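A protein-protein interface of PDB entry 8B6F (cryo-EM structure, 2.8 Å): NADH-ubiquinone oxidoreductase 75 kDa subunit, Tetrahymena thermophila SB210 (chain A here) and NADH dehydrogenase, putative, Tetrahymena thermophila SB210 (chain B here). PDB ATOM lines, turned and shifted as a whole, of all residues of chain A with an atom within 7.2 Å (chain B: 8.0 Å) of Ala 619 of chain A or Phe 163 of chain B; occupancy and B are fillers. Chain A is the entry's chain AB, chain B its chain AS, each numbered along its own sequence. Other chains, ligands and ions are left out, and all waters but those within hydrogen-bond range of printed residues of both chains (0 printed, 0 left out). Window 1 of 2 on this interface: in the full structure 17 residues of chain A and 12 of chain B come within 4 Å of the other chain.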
ATOM      1  N   TRP A 320      27.744  11.350  28.550  1.00  0.00           N
ATOM      2  CA  TRP A 320      27.180  11.369  27.205  1.00  0.00           C
ATOM      3  C   TRP A 320      25.903  10.545  27.139  1.00  0.00           C
ATOM      4  O   TRP A 320      24.932  10.940  26.483  1.00  0.00           O
ATOM      5  CB  TRP A 320      28.202  10.847  26.197  1.00  0.00           C
ATOM      6  CG  TRP A 320      29.225  11.854  25.803  1.00  0.00           C
ATOM      7  CD1 TRP A 320      30.504  11.946  26.261  1.00  0.00           C
ATOM      8  CD2 TRP A 320      29.057  12.918  24.861  1.00  0.00           C
ATOM      9  NE1 TRP A 320      31.145  13.003  25.663  1.00  0.00           N
ATOM     10  CE2 TRP A 320      30.277  13.616  24.799  1.00  0.00           C
ATOM     11  CE3 TRP A 320      27.991  13.347  24.063  1.00  0.00           C
ATOM     12  CZ2 TRP A 320      30.463  14.720  23.972  1.00  0.00           C
ATOM     13  CZ3 TRP A 320      28.176  14.445  23.241  1.00  0.00           C
ATOM     14  CH2 TRP A 320      29.403  15.119  23.202  1.00  0.00           C
ATOM     15  N   GLU A 321      25.880   9.397  27.818  1.00  0.00           N
ATOM     16  CA  GLU A 321      24.689   8.555  27.804  1.00  0.00           C
ATOM     17  C   GLU A 321      23.494   9.302  28.381  1.00  0.00           C
ATOM     18  O   GLU A 321      22.404   9.297  27.799  1.00  0.00           O
ATOM     19  CB  GLU A 321      24.952   7.264  28.580  1.00  0.00           C
ATOM     20  CG  GLU A 321      23.809   6.261  28.512  1.00  0.00           C
ATOM     21  CD  GLU A 321      24.168   4.923  29.133  1.00  0.00           C
ATOM     22  OE1 GLU A 321      25.328   4.757  29.562  1.00  0.00           O
ATOM     23  OE2 GLU A 321      23.289   4.037  29.192  1.00  0.00           O
ATOM     24  N   ILE A 324      22.418  12.190  25.925  1.00  0.00           N
ATOM     25  CA  ILE A 324      21.759  11.707  24.717  1.00  0.00           C
ATOM     26  C   ILE A 324      20.387  11.138  25.048  1.00  0.00           C
ATOM     27  O   ILE A 324      19.425  11.323  24.293  1.00  0.00           O
ATOM     28  CB  ILE A 324      22.646  10.674  23.998  1.00  0.00           C
ATOM     29  CG1 ILE A 324      23.972  11.310  23.562  1.00  0.00           C
ATOM     30  CG2 ILE A 324      21.910  10.074  22.808  1.00  0.00           C
ATOM     31  CD1 ILE A 324      23.845  12.352  22.467  1.00  0.00           C
ATOM     32  N   SER A 328      16.962  12.541  23.498  1.00  0.00           N
ATOM     33  CA  SER A 328      16.090  11.660  22.728  1.00  0.00           C
ATOM     34  C   SER A 328      14.680  11.645  23.304  1.00  0.00           C
ATOM     35  O   SER A 328      13.697  11.654  22.555  1.00  0.00           O
ATOM     36  CB  SER A 328      16.668  10.246  22.690  1.00  0.00           C
ATOM     37  OG  SER A 328      16.742   9.689  23.989  1.00  0.00           O
ATOM     38  N   PHE A 358      18.972  13.597  10.465  1.00  0.00           N
ATOM     39  CA  PHE A 358      18.272  13.376  11.725  1.00  0.00           C
ATOM     40  C   PHE A 358      16.968  14.162  11.771  1.00  0.00           C
ATOM     41  O   PHE A 358      15.924  13.632  12.164  1.00  0.00           O
ATOM     42  CB  PHE A 358      19.183  13.761  12.891  1.00  0.00           C
ATOM     43  CG  PHE A 358      18.523  13.674  14.233  1.00  0.00           C
ATOM     44  CD1 PHE A 358      18.218  12.446  14.791  1.00  0.00           C
ATOM     45  CD2 PHE A 358      18.232  14.823  14.949  1.00  0.00           C
ATOM     46  CE1 PHE A 358      17.616  12.365  16.031  1.00  0.00           C
ATOM     47  CE2 PHE A 358      17.632  14.748  16.188  1.00  0.00           C
ATOM     48  CZ  PHE A 358      17.326  13.517  16.730  1.00  0.00           C
ATOM     49  N   ASP A 609      36.496  15.349  26.784  1.00  0.00           N
ATOM     50  CA  ASP A 609      35.523  14.341  26.389  1.00  0.00           C
ATOM     51  C   ASP A 609      34.751  14.740  25.138  1.00  0.00           C
ATOM     52  O   ASP A 609      33.705  14.152  24.847  1.00  0.00           O
ATOM     53  CB  ASP A 609      34.555  14.073  27.541  1.00  0.00           C
ATOM     54  CG  ASP A 609      33.915  12.702  27.460  1.00  0.00           C
ATOM     55  OD1 ASP A 609      33.896  12.114  26.358  1.00  0.00           O
ATOM     56  OD2 ASP A 609      33.431  12.208  28.499  1.00  0.00           O
ATOM     57  N   ALA A 610      35.239  15.732  24.399  1.00  0.00           N
ATOM     58  CA  ALA A 610      34.534  16.189  23.211  1.00  0.00           C
ATOM     59  C   ALA A 610      34.462  15.083  22.166  1.00  0.00           C
ATOM     60  O   ALA A 610      35.390  14.285  22.014  1.00  0.00           O
ATOM     61  CB  ALA A 610      35.229  17.422  22.631  1.00  0.00           C
ATOM     62  N   ARG A 611      33.345  15.042  21.445  1.00  0.00           N
ATOM     63  CA  ARG A 611      33.116  14.077  20.383  1.00  0.00           C
ATOM     64  C   ARG A 611      32.814  14.815  19.087  1.00  0.00           C
ATOM     65  O   ARG A 611      32.340  15.955  19.100  1.00  0.00           O
ATOM     66  CB  ARG A 611      31.948  13.141  20.716  1.00  0.00           C
ATOM     67  CG  ARG A 611      32.154  12.282  21.949  1.00  0.00           C
ATOM     68  CD  ARG A 611      33.150  11.167  21.693  1.00  0.00           C
ATOM     69  NE  ARG A 611      33.052  10.122  22.703  1.00  0.00           N
ATOM     70  CZ  ARG A 611      33.614  10.181  23.902  1.00  0.00           C
ATOM     71  NH1 ARG A 611      34.332  11.225  24.279  1.00  0.00           N
ATOM     72  NH2 ARG A 611      33.448   9.168  24.746  1.00  0.00           N
ATOM     73  N   GLU A 612      33.094  14.160  17.963  1.00  0.00           N
ATOM     74  CA  GLU A 612      32.763  14.743  16.673  1.00  0.00           C
ATOM     75  C   GLU A 612      31.258  14.955  16.566  1.00  0.00           C
ATOM     76  O   GLU A 612      30.462  14.112  16.988  1.00  0.00           O
ATOM     77  CB  GLU A 612      33.253  13.846  15.537  1.00  0.00           C
ATOM     78  CG  GLU A 612      34.763  13.713  15.472  1.00  0.00           C
ATOM     79  CD  GLU A 612      35.229  12.978  14.231  1.00  0.00           C
ATOM     80  OE1 GLU A 612      34.388  12.696  13.354  1.00  0.00           O
ATOM     81  OE2 GLU A 612      36.439  12.684  14.132  1.00  0.00           O
ATOM     82  N   ASP A 613      30.871  16.092  15.986  1.00  0.00           N
ATOM     83  CA  ASP A 613      29.457  16.455  15.950  1.00  0.00           C
ATOM     84  C   ASP A 613      28.639  15.445  15.154  1.00  0.00           C
ATOM     85  O   ASP A 613      27.514  15.111  15.541  1.00  0.00           O
ATOM     86  CB  ASP A 613      29.288  17.863  15.377  1.00  0.00           C
ATOM     87  CG  ASP A 613      30.199  18.129  14.199  1.00  0.00           C
ATOM     88  OD1 ASP A 613      30.824  17.168  13.701  1.00  0.00           O
ATOM     89  OD2 ASP A 613      30.300  19.300  13.777  1.00  0.00           O
ATOM     90  N   TRP A 614      29.179  14.947  14.041  1.00  0.00           N
ATOM     91  CA  TRP A 614      28.438  13.959  13.263  1.00  0.00           C
ATOM     92  C   TRP A 614      28.256  12.670  14.057  1.00  0.00           C
ATOM     93  O   TRP A 614      27.197  12.038  13.988  1.00  0.00           O
ATOM     94  CB  TRP A 614      29.136  13.690  11.929  1.00  0.00           C
ATOM     95  CG  TRP A 614      30.315  12.775  12.004  1.00  0.00           C
ATOM     96  CD1 TRP A 614      31.621  13.133  12.146  1.00  0.00           C
ATOM     97  CD2 TRP A 614      30.295  11.345  11.928  1.00  0.00           C
ATOM     98  NE1 TRP A 614      32.418  12.014  12.168  1.00  0.00           N
ATOM     99  CE2 TRP A 614      31.628  10.903  12.036  1.00  0.00           C
ATOM    100  CE3 TRP A 614      29.279  10.394  11.783  1.00  0.00           C
ATOM    101  CZ2 TRP A 614      31.972   9.554  12.003  1.00  0.00           C
ATOM    102  CZ3 TRP A 614      29.622   9.054  11.750  1.00  0.00           C
ATOM    103  CH2 TRP A 614      30.958   8.646  11.861  1.00  0.00           C
ATOM    104  N   GLN A 615      29.278  12.261  14.811  1.00  0.00           N
ATOM    105  CA  GLN A 615      29.134  11.093  15.674  1.00  0.00           C
ATOM    106  C   GLN A 615      28.083  11.334  16.750  1.00  0.00           C
ATOM    107  O   GLN A 615      27.297  10.437  17.072  1.00  0.00           O
ATOM    108  CB  GLN A 615      30.475  10.734  16.313  1.00  0.00           C
ATOM    109  CG  GLN A 615      31.521  10.270  15.319  1.00  0.00           C
ATOM    110  CD  GLN A 615      32.720   9.640  15.993  1.00  0.00           C
ATOM    111  OE1 GLN A 615      32.823   9.628  17.217  1.00  0.00           O
ATOM    112  NE2 GLN A 615      33.634   9.105  15.191  1.00  0.00           N
ATOM    113  N   ILE A 616      28.057  12.538  17.324  1.00  0.00           N
ATOM    114  CA  ILE A 616      27.052  12.855  18.335  1.00  0.00           C
ATOM    115  C   ILE A 616      25.655  12.739  17.743  1.00  0.00           C
ATOM    116  O   ILE A 616      24.747  12.173  18.361  1.00  0.00           O
ATOM    117  CB  ILE A 616      27.305  14.258  18.916  1.00  0.00           C
ATOM    118  CG1 ILE A 616      28.642  14.294  19.656  1.00  0.00           C
ATOM    119  CG2 ILE A 616      26.175  14.662  19.858  1.00  0.00           C
ATOM    120  CD1 ILE A 616      29.120  15.691  19.980  1.00  0.00           C
ATOM    121  N   ILE A 617      25.460  13.277  16.539  1.00  0.00           N
ATOM    122  CA  ILE A 617      24.150  13.217  15.900  1.00  0.00           C
ATOM    123  C   ILE A 617      23.781  11.773  15.583  1.00  0.00           C
ATOM    124  O   ILE A 617      22.620  11.372  15.718  1.00  0.00           O
ATOM    125  CB  ILE A 617      24.136  14.104  14.644  1.00  0.00           C
ATOM    126  CG1 ILE A 617      24.308  15.573  15.043  1.00  0.00           C
ATOM    127  CG2 ILE A 617      22.837  13.914  13.869  1.00  0.00           C
ATOM    128  CD1 ILE A 617      24.540  16.508  13.877  1.00  0.00           C
ATOM    129  N   ARG A 618      24.756  10.974  15.147  1.00  0.00           N
ATOM    130  CA  ARG A 618      24.490   9.568  14.866  1.00  0.00           C
ATOM    131  C   ARG A 618      24.048   8.838  16.128  1.00  0.00           C
ATOM    132  O   ARG A 618      23.079   8.070  16.109  1.00  0.00           O
ATOM    133  CB  ARG A 618      25.739   8.923  14.262  1.00  0.00           C
ATOM    134  CG  ARG A 618      25.716   7.404  14.183  1.00  0.00           C
ATOM    135  CD  ARG A 618      24.562   6.898  13.340  1.00  0.00           C
ATOM    136  NE  ARG A 618      24.691   5.475  13.049  1.00  0.00           N
ATOM    137  CZ  ARG A 618      24.468   4.506  13.926  1.00  0.00           C
ATOM    138  NH1 ARG A 618      24.122   4.769  15.174  1.00  0.00           N
ATOM    139  NH2 ARG A 618      24.599   3.241  13.540  1.00  0.00           N
ATOM    140  N   ALA A 619      24.753   9.059  17.238  1.00  0.00           N
ATOM    141  CA  ALA A 619      24.373   8.421  18.495  1.00  0.00           C
ATOM    142  C   ALA A 619      22.997   8.885  18.955  1.00  0.00           C
ATOM    143  O   ALA A 619      22.187   8.081  19.433  1.00  0.00           O
ATOM    144  CB  ALA A 619      25.419   8.711  19.569  1.00  0.00           C
ATOM    145  N   LEU A 620      22.713  10.181  18.817  1.00  0.00           N
ATOM    146  CA  LEU A 620      21.408  10.706  19.208  1.00  0.00           C
ATOM    147  C   LEU A 620      20.294  10.082  18.381  1.00  0.00           C
ATOM    148  O   LEU A 620      19.238   9.725  18.915  1.00  0.00           O
ATOM    149  CB  LEU A 620      21.390  12.226  19.070  1.00  0.00           C
ATOM    150  CG  LEU A 620      20.024  12.900  19.230  1.00  0.00           C
ATOM    151  CD1 LEU A 620      19.368  12.503  20.541  1.00  0.00           C
ATOM    152  CD2 LEU A 620      20.169  14.412  19.141  1.00  0.00           C
ATOM    153  N   SER A 621      20.509   9.946  17.074  1.00  0.00           N
ATOM    154  CA  SER A 621      19.500   9.324  16.226  1.00  0.00           C
ATOM    155  C   SER A 621      19.260   7.875  16.624  1.00  0.00           C
ATOM    156  O   SER A 621      18.110   7.430  16.707  1.00  0.00           O
ATOM    157  CB  SER A 621      19.947   9.399  14.771  1.00  0.00           C
ATOM    158  OG  SER A 621      21.092   8.583  14.593  1.00  0.00           O
ATOM    159  N   GLU A 622      20.331   7.119  16.870  1.00  0.00           N
ATOM    160  CA  GLU A 622      20.162   5.721  17.250  1.00  0.00           C
ATOM    161  C   GLU A 622      19.398   5.598  18.562  1.00  0.00           C
ATOM    162  O   GLU A 622      18.515   4.743  18.697  1.00  0.00           O
ATOM    163  CB  GLU A 622      21.521   5.034  17.359  1.00  0.00           C
ATOM    164  CG  GLU A 622      21.422   3.565  17.737  1.00  0.00           C
ATOM    165  CD  GLU A 622      22.765   2.870  17.738  1.00  0.00           C
ATOM    166  OE1 GLU A 622      23.746   3.469  17.254  1.00  0.00           O
ATOM    167  OE2 GLU A 622      22.839   1.723  18.225  1.00  0.00           O
ATOM    168  N   GLU A 623      19.728   6.440  19.542  1.00  0.00           N
ATOM    169  CA  GLU A 623      19.025   6.396  20.819  1.00  0.00           C
ATOM    170  C   GLU A 623      17.565   6.796  20.656  1.00  0.00           C
ATOM    171  O   GLU A 623      16.678   6.196  21.275  1.00  0.00           O
ATOM    172  CB  GLU A 623      19.721   7.304  21.832  1.00  0.00           C
ATOM    173  CG  GLU A 623      20.990   6.711  22.423  1.00  0.00           C
ATOM    174  CD  GLU A 623      20.715   5.546  23.352  1.00  0.00           C
ATOM    175  OE1 GLU A 623      19.539   5.150  23.482  1.00  0.00           O
ATOM    176  OE2 GLU A 623      21.675   5.028  23.960  1.00  0.00           O
ATOM    177  N   ALA A 624      17.292   7.808  19.833  1.00  0.00           N
ATOM    178  CA  ALA A 624      15.917   8.231  19.604  1.00  0.00           C
ATOM    179  C   ALA A 624      15.127   7.216  18.791  1.00  0.00           C
ATOM    180  O   ALA A 624      13.895   7.299  18.749  1.00  0.00           O
ATOM    181  CB  ALA A 624      15.894   9.586  18.896  1.00  0.00           C
ATOM    182  N   GLY A 625      15.799   6.273  18.142  1.00  0.00           N
ATOM    183  CA  GLY A 625      15.131   5.222  17.407  1.00  0.00           C
ATOM    184  C   GLY A 625      15.042   5.434  15.914  1.00  0.00           C
ATOM    185  O   GLY A 625      14.226   4.770  15.264  1.00  0.00           O
ATOM    186  N   LEU A 628      20.809   6.304  11.653  1.00  0.00           N
ATOM    187  CA  LEU A 628      21.282   6.778  10.364  1.00  0.00           C
ATOM    188  C   LEU A 628      22.092   5.689   9.666  1.00  0.00           C
ATOM    189  O   LEU A 628      22.687   4.831  10.325  1.00  0.00           O
ATOM    190  CB  LEU A 628      22.137   8.028  10.534  1.00  0.00           C
ATOM    191  CG  LEU A 628      21.435   9.191  11.239  1.00  0.00           C
ATOM    192  CD1 LEU A 628      22.423  10.273  11.623  1.00  0.00           C
ATOM    193  CD2 LEU A 628      20.348   9.769  10.354  1.00  0.00           C
ATOM    194  N   TYR B 153      24.604  -1.764  27.267  1.00  0.00           N
ATOM    195  CA  TYR B 153      24.471  -1.484  25.843  1.00  0.00           C
ATOM    196  C   TYR B 153      23.834  -2.646  25.086  1.00  0.00           C
ATOM    197  O   TYR B 153      24.185  -2.909  23.934  1.00  0.00           O
ATOM    198  CB  TYR B 153      25.834  -1.150  25.238  1.00  0.00           C
ATOM    199  CG  TYR B 153      26.587  -0.066  25.978  1.00  0.00           C
ATOM    200  CD1 TYR B 153      25.913   0.931  26.670  1.00  0.00           C
ATOM    201  CD2 TYR B 153      27.974  -0.039  25.977  1.00  0.00           C
ATOM    202  CE1 TYR B 153      26.599   1.921  27.345  1.00  0.00           C
ATOM    203  CE2 TYR B 153      28.671   0.947  26.649  1.00  0.00           C
ATOM    204  CZ  TYR B 153      27.977   1.924  27.330  1.00  0.00           C
ATOM    205  OH  TYR B 153      28.666   2.907  28.000  1.00  0.00           O
ATOM    206  N   SER B 157      24.292  -0.655  18.630  1.00  0.00           N
ATOM    207  CA  SER B 157      25.305  -0.831  17.601  1.00  0.00           C
ATOM    208  C   SER B 157      26.701  -0.682  18.194  1.00  0.00           C
ATOM    209  O   SER B 157      26.912   0.031  19.177  1.00  0.00           O
ATOM    210  CB  SER B 157      25.104   0.177  16.472  1.00  0.00           C
ATOM    211  OG  SER B 157      25.217   1.506  16.947  1.00  0.00           O
ATOM    212  N   LYS B 158      27.663  -1.375  17.579  1.00  0.00           N
ATOM    213  CA  LYS B 158      29.052  -1.251  18.010  1.00  0.00           C
ATOM    214  C   LYS B 158      29.527   0.193  17.950  1.00  0.00           C
ATOM    215  O   LYS B 158      30.349   0.611  18.773  1.00  0.00           O
ATOM    216  CB  LYS B 158      29.950  -2.141  17.150  1.00  0.00           C
ATOM    217  CG  LYS B 158      29.590  -3.619  17.218  1.00  0.00           C
ATOM    218  CD  LYS B 158      30.531  -4.474  16.378  1.00  0.00           C
ATOM    219  CE  LYS B 158      30.374  -4.191  14.891  1.00  0.00           C
ATOM    220  NZ  LYS B 158      31.190  -5.120  14.059  1.00  0.00           N
ATOM    221  N   PHE B 159      29.029   0.970  16.986  1.00  0.00           N
ATOM    222  CA  PHE B 159      29.391   2.380  16.916  1.00  0.00           C
ATOM    223  C   PHE B 159      28.961   3.115  18.177  1.00  0.00           C
ATOM    224  O   PHE B 159      29.735   3.884  18.758  1.00  0.00           O
ATOM    225  CB  PHE B 159      28.757   3.027  15.685  1.00  0.00           C
ATOM    226  CG  PHE B 159      28.922   4.519  15.639  1.00  0.00           C
ATOM    227  CD1 PHE B 159      27.984   5.354  16.227  1.00  0.00           C
ATOM    228  CD2 PHE B 159      30.017   5.087  15.012  1.00  0.00           C
ATOM    229  CE1 PHE B 159      28.137   6.724  16.190  1.00  0.00           C
ATOM    230  CE2 PHE B 159      30.176   6.457  14.971  1.00  0.00           C
ATOM    231  CZ  PHE B 159      29.233   7.277  15.560  1.00  0.00           C
ATOM    232  N   LEU B 160      27.721   2.893  18.617  1.00  0.00           N
ATOM    233  CA  LEU B 160      27.237   3.563  19.818  1.00  0.00           C
ATOM    234  C   LEU B 160      27.985   3.081  21.054  1.00  0.00           C
ATOM    235  O   LEU B 160      28.288   3.874  21.952  1.00  0.00           O
ATOM    236  CB  LEU B 160      25.734   3.335  19.969  1.00  0.00           C
ATOM    237  CG  LEU B 160      25.036   4.068  21.114  1.00  0.00           C
ATOM    238  CD1 LEU B 160      25.277   5.565  21.027  1.00  0.00           C
ATOM    239  CD2 LEU B 160      23.550   3.771  21.090  1.00  0.00           C
ATOM    240  N   GLN B 161      28.285   1.783  21.122  1.00  0.00           N
ATOM    241  CA  GLN B 161      29.062   1.264  22.241  1.00  0.00           C
ATOM    242  C   GLN B 161      30.420   1.951  22.315  1.00  0.00           C
ATOM    243  O   GLN B 161      30.853   2.387  23.387  1.00  0.00           O
ATOM    244  CB  GLN B 161      29.228  -0.250  22.106  1.00  0.00           C
ATOM    245  CG  GLN B 161      27.919  -1.016  22.184  1.00  0.00           C
ATOM    246  CD  GLN B 161      28.097  -2.499  21.934  1.00  0.00           C
ATOM    247  OE1 GLN B 161      29.202  -2.967  21.664  1.00  0.00           O
ATOM    248  NE2 GLN B 161      27.005  -3.249  22.024  1.00  0.00           N
ATOM    249  N   GLY B 162      31.106   2.055  21.178  1.00  0.00           N
ATOM    250  CA  GLY B 162      32.392   2.731  21.158  1.00  0.00           C
ATOM    251  C   GLY B 162      32.277   4.210  21.471  1.00  0.00           C
ATOM    252  O   GLY B 162      33.138   4.780  22.145  1.00  0.00           O
ATOM    253  N   PHE B 163      31.211   4.852  20.990  1.00  0.00           N
ATOM    254  CA  PHE B 163      31.008   6.267  21.279  1.00  0.00           C
ATOM    255  C   PHE B 163      30.877   6.509  22.776  1.00  0.00           C
ATOM    256  O   PHE B 163      31.474   7.447  23.315  1.00  0.00           O
ATOM    257  CB  PHE B 163      29.766   6.769  20.539  1.00  0.00           C
ATOM    258  CG  PHE B 163      29.414   8.197  20.836  1.00  0.00           C
ATOM    259  CD1 PHE B 163      29.941   9.227  20.077  1.00  0.00           C
ATOM    260  CD2 PHE B 163      28.541   8.509  21.865  1.00  0.00           C
ATOM    261  CE1 PHE B 163      29.615  10.543  20.345  1.00  0.00           C
ATOM    262  CE2 PHE B 163      28.211   9.822  22.139  1.00  0.00           C
ATOM    263  CZ  PHE B 163      28.747  10.839  21.377  1.00  0.00           C
ATOM    264  N   TYR B 164      30.101   5.673  23.467  1.00  0.00           N
ATOM    265  CA  TYR B 164      29.955   5.832  24.910  1.00  0.00           C
ATOM    266  C   TYR B 164      31.239   5.462  25.643  1.00  0.00           C
ATOM    267  O   TYR B 164      31.601   6.106  26.634  1.00  0.00           O
ATOM    268  CB  TYR B 164      28.788   4.980  25.413  1.00  0.00           C
ATOM    269  CG  TYR B 164      27.416   5.524  25.070  1.00  0.00           C
ATOM    270  CD1 TYR B 164      27.162   6.889  25.070  1.00  0.00           C
ATOM    271  CD2 TYR B 164      26.373   4.665  24.751  1.00  0.00           C
ATOM    272  CE1 TYR B 164      25.912   7.383  24.761  1.00  0.00           C
ATOM    273  CE2 TYR B 164      25.119   5.149  24.439  1.00  0.00           C
ATOM    274  CZ  TYR B 164      24.895   6.509  24.446  1.00  0.00           C
ATOM    275  OH  TYR B 164      23.647   6.995  24.137  1.00  0.00           O
ATOM    276  N   LYS B 165      31.943   4.430  25.173  1.00  0.00           N
ATOM    277  CA  LYS B 165      33.175   4.020  25.837  1.00  0.00           C
ATOM    278  C   LYS B 165      34.238   5.107  25.752  1.00  0.00           C
ATOM    279  O   LYS B 165      34.935   5.382  26.734  1.00  0.00           O
ATOM    280  CB  LYS B 165      33.694   2.721  25.219  1.00  0.00           C
ATOM    281  CG  LYS B 165      32.814   1.509  25.484  1.00  0.00           C
ATOM    282  CD  LYS B 165      33.080   0.404  24.470  1.00  0.00           C
ATOM    283  CE  LYS B 165      32.164  -0.789  24.700  1.00  0.00           C
ATOM    284  NZ  LYS B 165      32.351  -1.846  23.664  1.00  0.00           N
ATOM    285  N   GLY B 166      34.376   5.733  24.590  1.00  0.00           N
ATOM    286  CA  GLY B 166      35.420   6.711  24.369  1.00  0.00           C
ATOM    287  C   GLY B 166      36.700   6.085  23.843  1.00  0.00           C
ATOM    288  O   GLY B 166      36.921   4.879  23.922  1.00  0.00           O
ATOM    289  N   ASN B 167      37.563   6.944  23.289  1.00  0.00           N
ATOM    290  CA  ASN B 167      38.825   6.482  22.726  1.00  0.00           C
ATOM    291  C   ASN B 167      39.990   7.397  23.095  1.00  0.00           C
ATOM    292  O   ASN B 167      41.010   7.397  22.396  1.00  0.00           O
ATOM    293  CB  ASN B 167      38.731   6.367  21.203  1.00  0.00           C
ATOM    294  CG  ASN B 167      38.510   7.705  20.533  1.00  0.00           C
ATOM    295  OD1 ASN B 167      37.902   8.606  21.107  1.00  0.00           O
ATOM    296  ND2 ASN B 167      39.007   7.842  19.310  1.00  0.00           N
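O of Phe 163 of chain B sits at hydrogen-bond distance from NH2 of Arg 611 of chain A (3.0 Å).
The side-chain carboxylate (OE1) of Glu 622 of chain A is in hydrogen-bond range of the side-chain hydroxyl (OG) of Ser 157 of chain B, 2.5 Å away.
OE2 of Glu 623 of chain A is in hydrogen-bond range of OH of Tyr 164 of chain B (2.8 Å).
The backbone carbonyl oxygen (O) of Ile 324 of chain A lies within hydrogen-bond range of the side-chain hydroxyl (OG) of Ser 328 of chain A (3.2 Å).
The side-chain carboxylate of Asp 609 of chain A lies within salt-bridge range of the guanidinium group of Arg 611 of chain A, at 3.4 Å.
The backbone carbonyl oxygen of Arg 618 of chain A is in hydrogen-bond range of the side-chain hydroxyl of Ser 621 of chain A, at 2.6 Å.
The guanidinium group (NH1) of Arg 618 of chain A lies within salt-bridge range of the side-chain carboxylate (OE1) of Glu 622 of chain A.
The side-chain amide nitrogen (NE2) of Gln 161 of chain B is in hydrogen-bond range of the backbone carbonyl oxygen (O) of Tyr 153 of chain B, 3.4 Å away.
OG of Ser 157 of chain B is in hydrogen-bond range of N of Leu 160 of chain B (3.3 Å).
Among the printed residues, pairs that only touch across the chains: Trp 320 of chain A with Phe 163 of chain B (3.8 Å), Trp 320 of chain A with Tyr 164 of chain B (3.96 Å), Glu 321 of chain A with Tyr 153 of chain B (3.8 Å), Glu 321 of chain A with Tyr 164 of chain B (3.5 Å), Ile 324 of chain A with Tyr 164 of chain B (3.8 Å), Arg 611 of chain A with Gly 166 of chain B (3.2 Å), Trp 614 of chain A with Phe 159 of chain B (3.9 Å), Gln 615 of chain A with Phe 159 of chain B (3.7 Å), Gln 615 of chain A with Phe 163 of chain B (3.99 Å), Ile 616 of chain A with Phe 163 of chain B (3.9 Å), Arg 618 of chain A with Ser 157 of chain B (3.9 Å), Arg 618 of chain A with Phe 159 of chain B (3.2 Å), Ala 619 of chain A with Leu 160 of chain B (3.5 Å), Ala 619 of chain A with Phe 163 of chain B (3.9 Å), Glu 622 of chain A with Leu 160 of chain B (3.4 Å) and Glu 623 of chain A with Leu 160 of chain B (3.7 Å).
Of the printed residues of chain B, Trp 320 of chain A touches Phe 163 and Tyr 164.
Ala 619 of chain A touches just these residues of chain B: Leu 160 (3.5 Å) and Phe 163 (3.9 Å).
Gly 625 of chain A touches none of the printed residues of chain B.
Of the printed residues of chain A, Leu 160 of chain B touches Ala 619, Glu 622 and Glu 623.
Of the printed residues of chain A, Phe 163 of chain B touches Trp 320 (3.8 Å), Arg 611 (3.0 Å), Gln 615 (3.99 Å), Ile 616 (3.9 Å) and Ala 619 (3.9 Å).
Lys 165 of chain B touches none of the printed residues of chain A.
The nearest residue of chain B that does not touch Ala 619 of chain A is Phe 159 of chain B (4.2 Å).
Of the 23 printed residues of chain A, 11 touch a printed residue of chain B.
Among the printed residues, 19 pairs touch across the chains.
Among the printed residues, no Asp or Glu carboxylate lies within 4 Å of a Lys or Arg side-chain nitrogen of the other chain.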
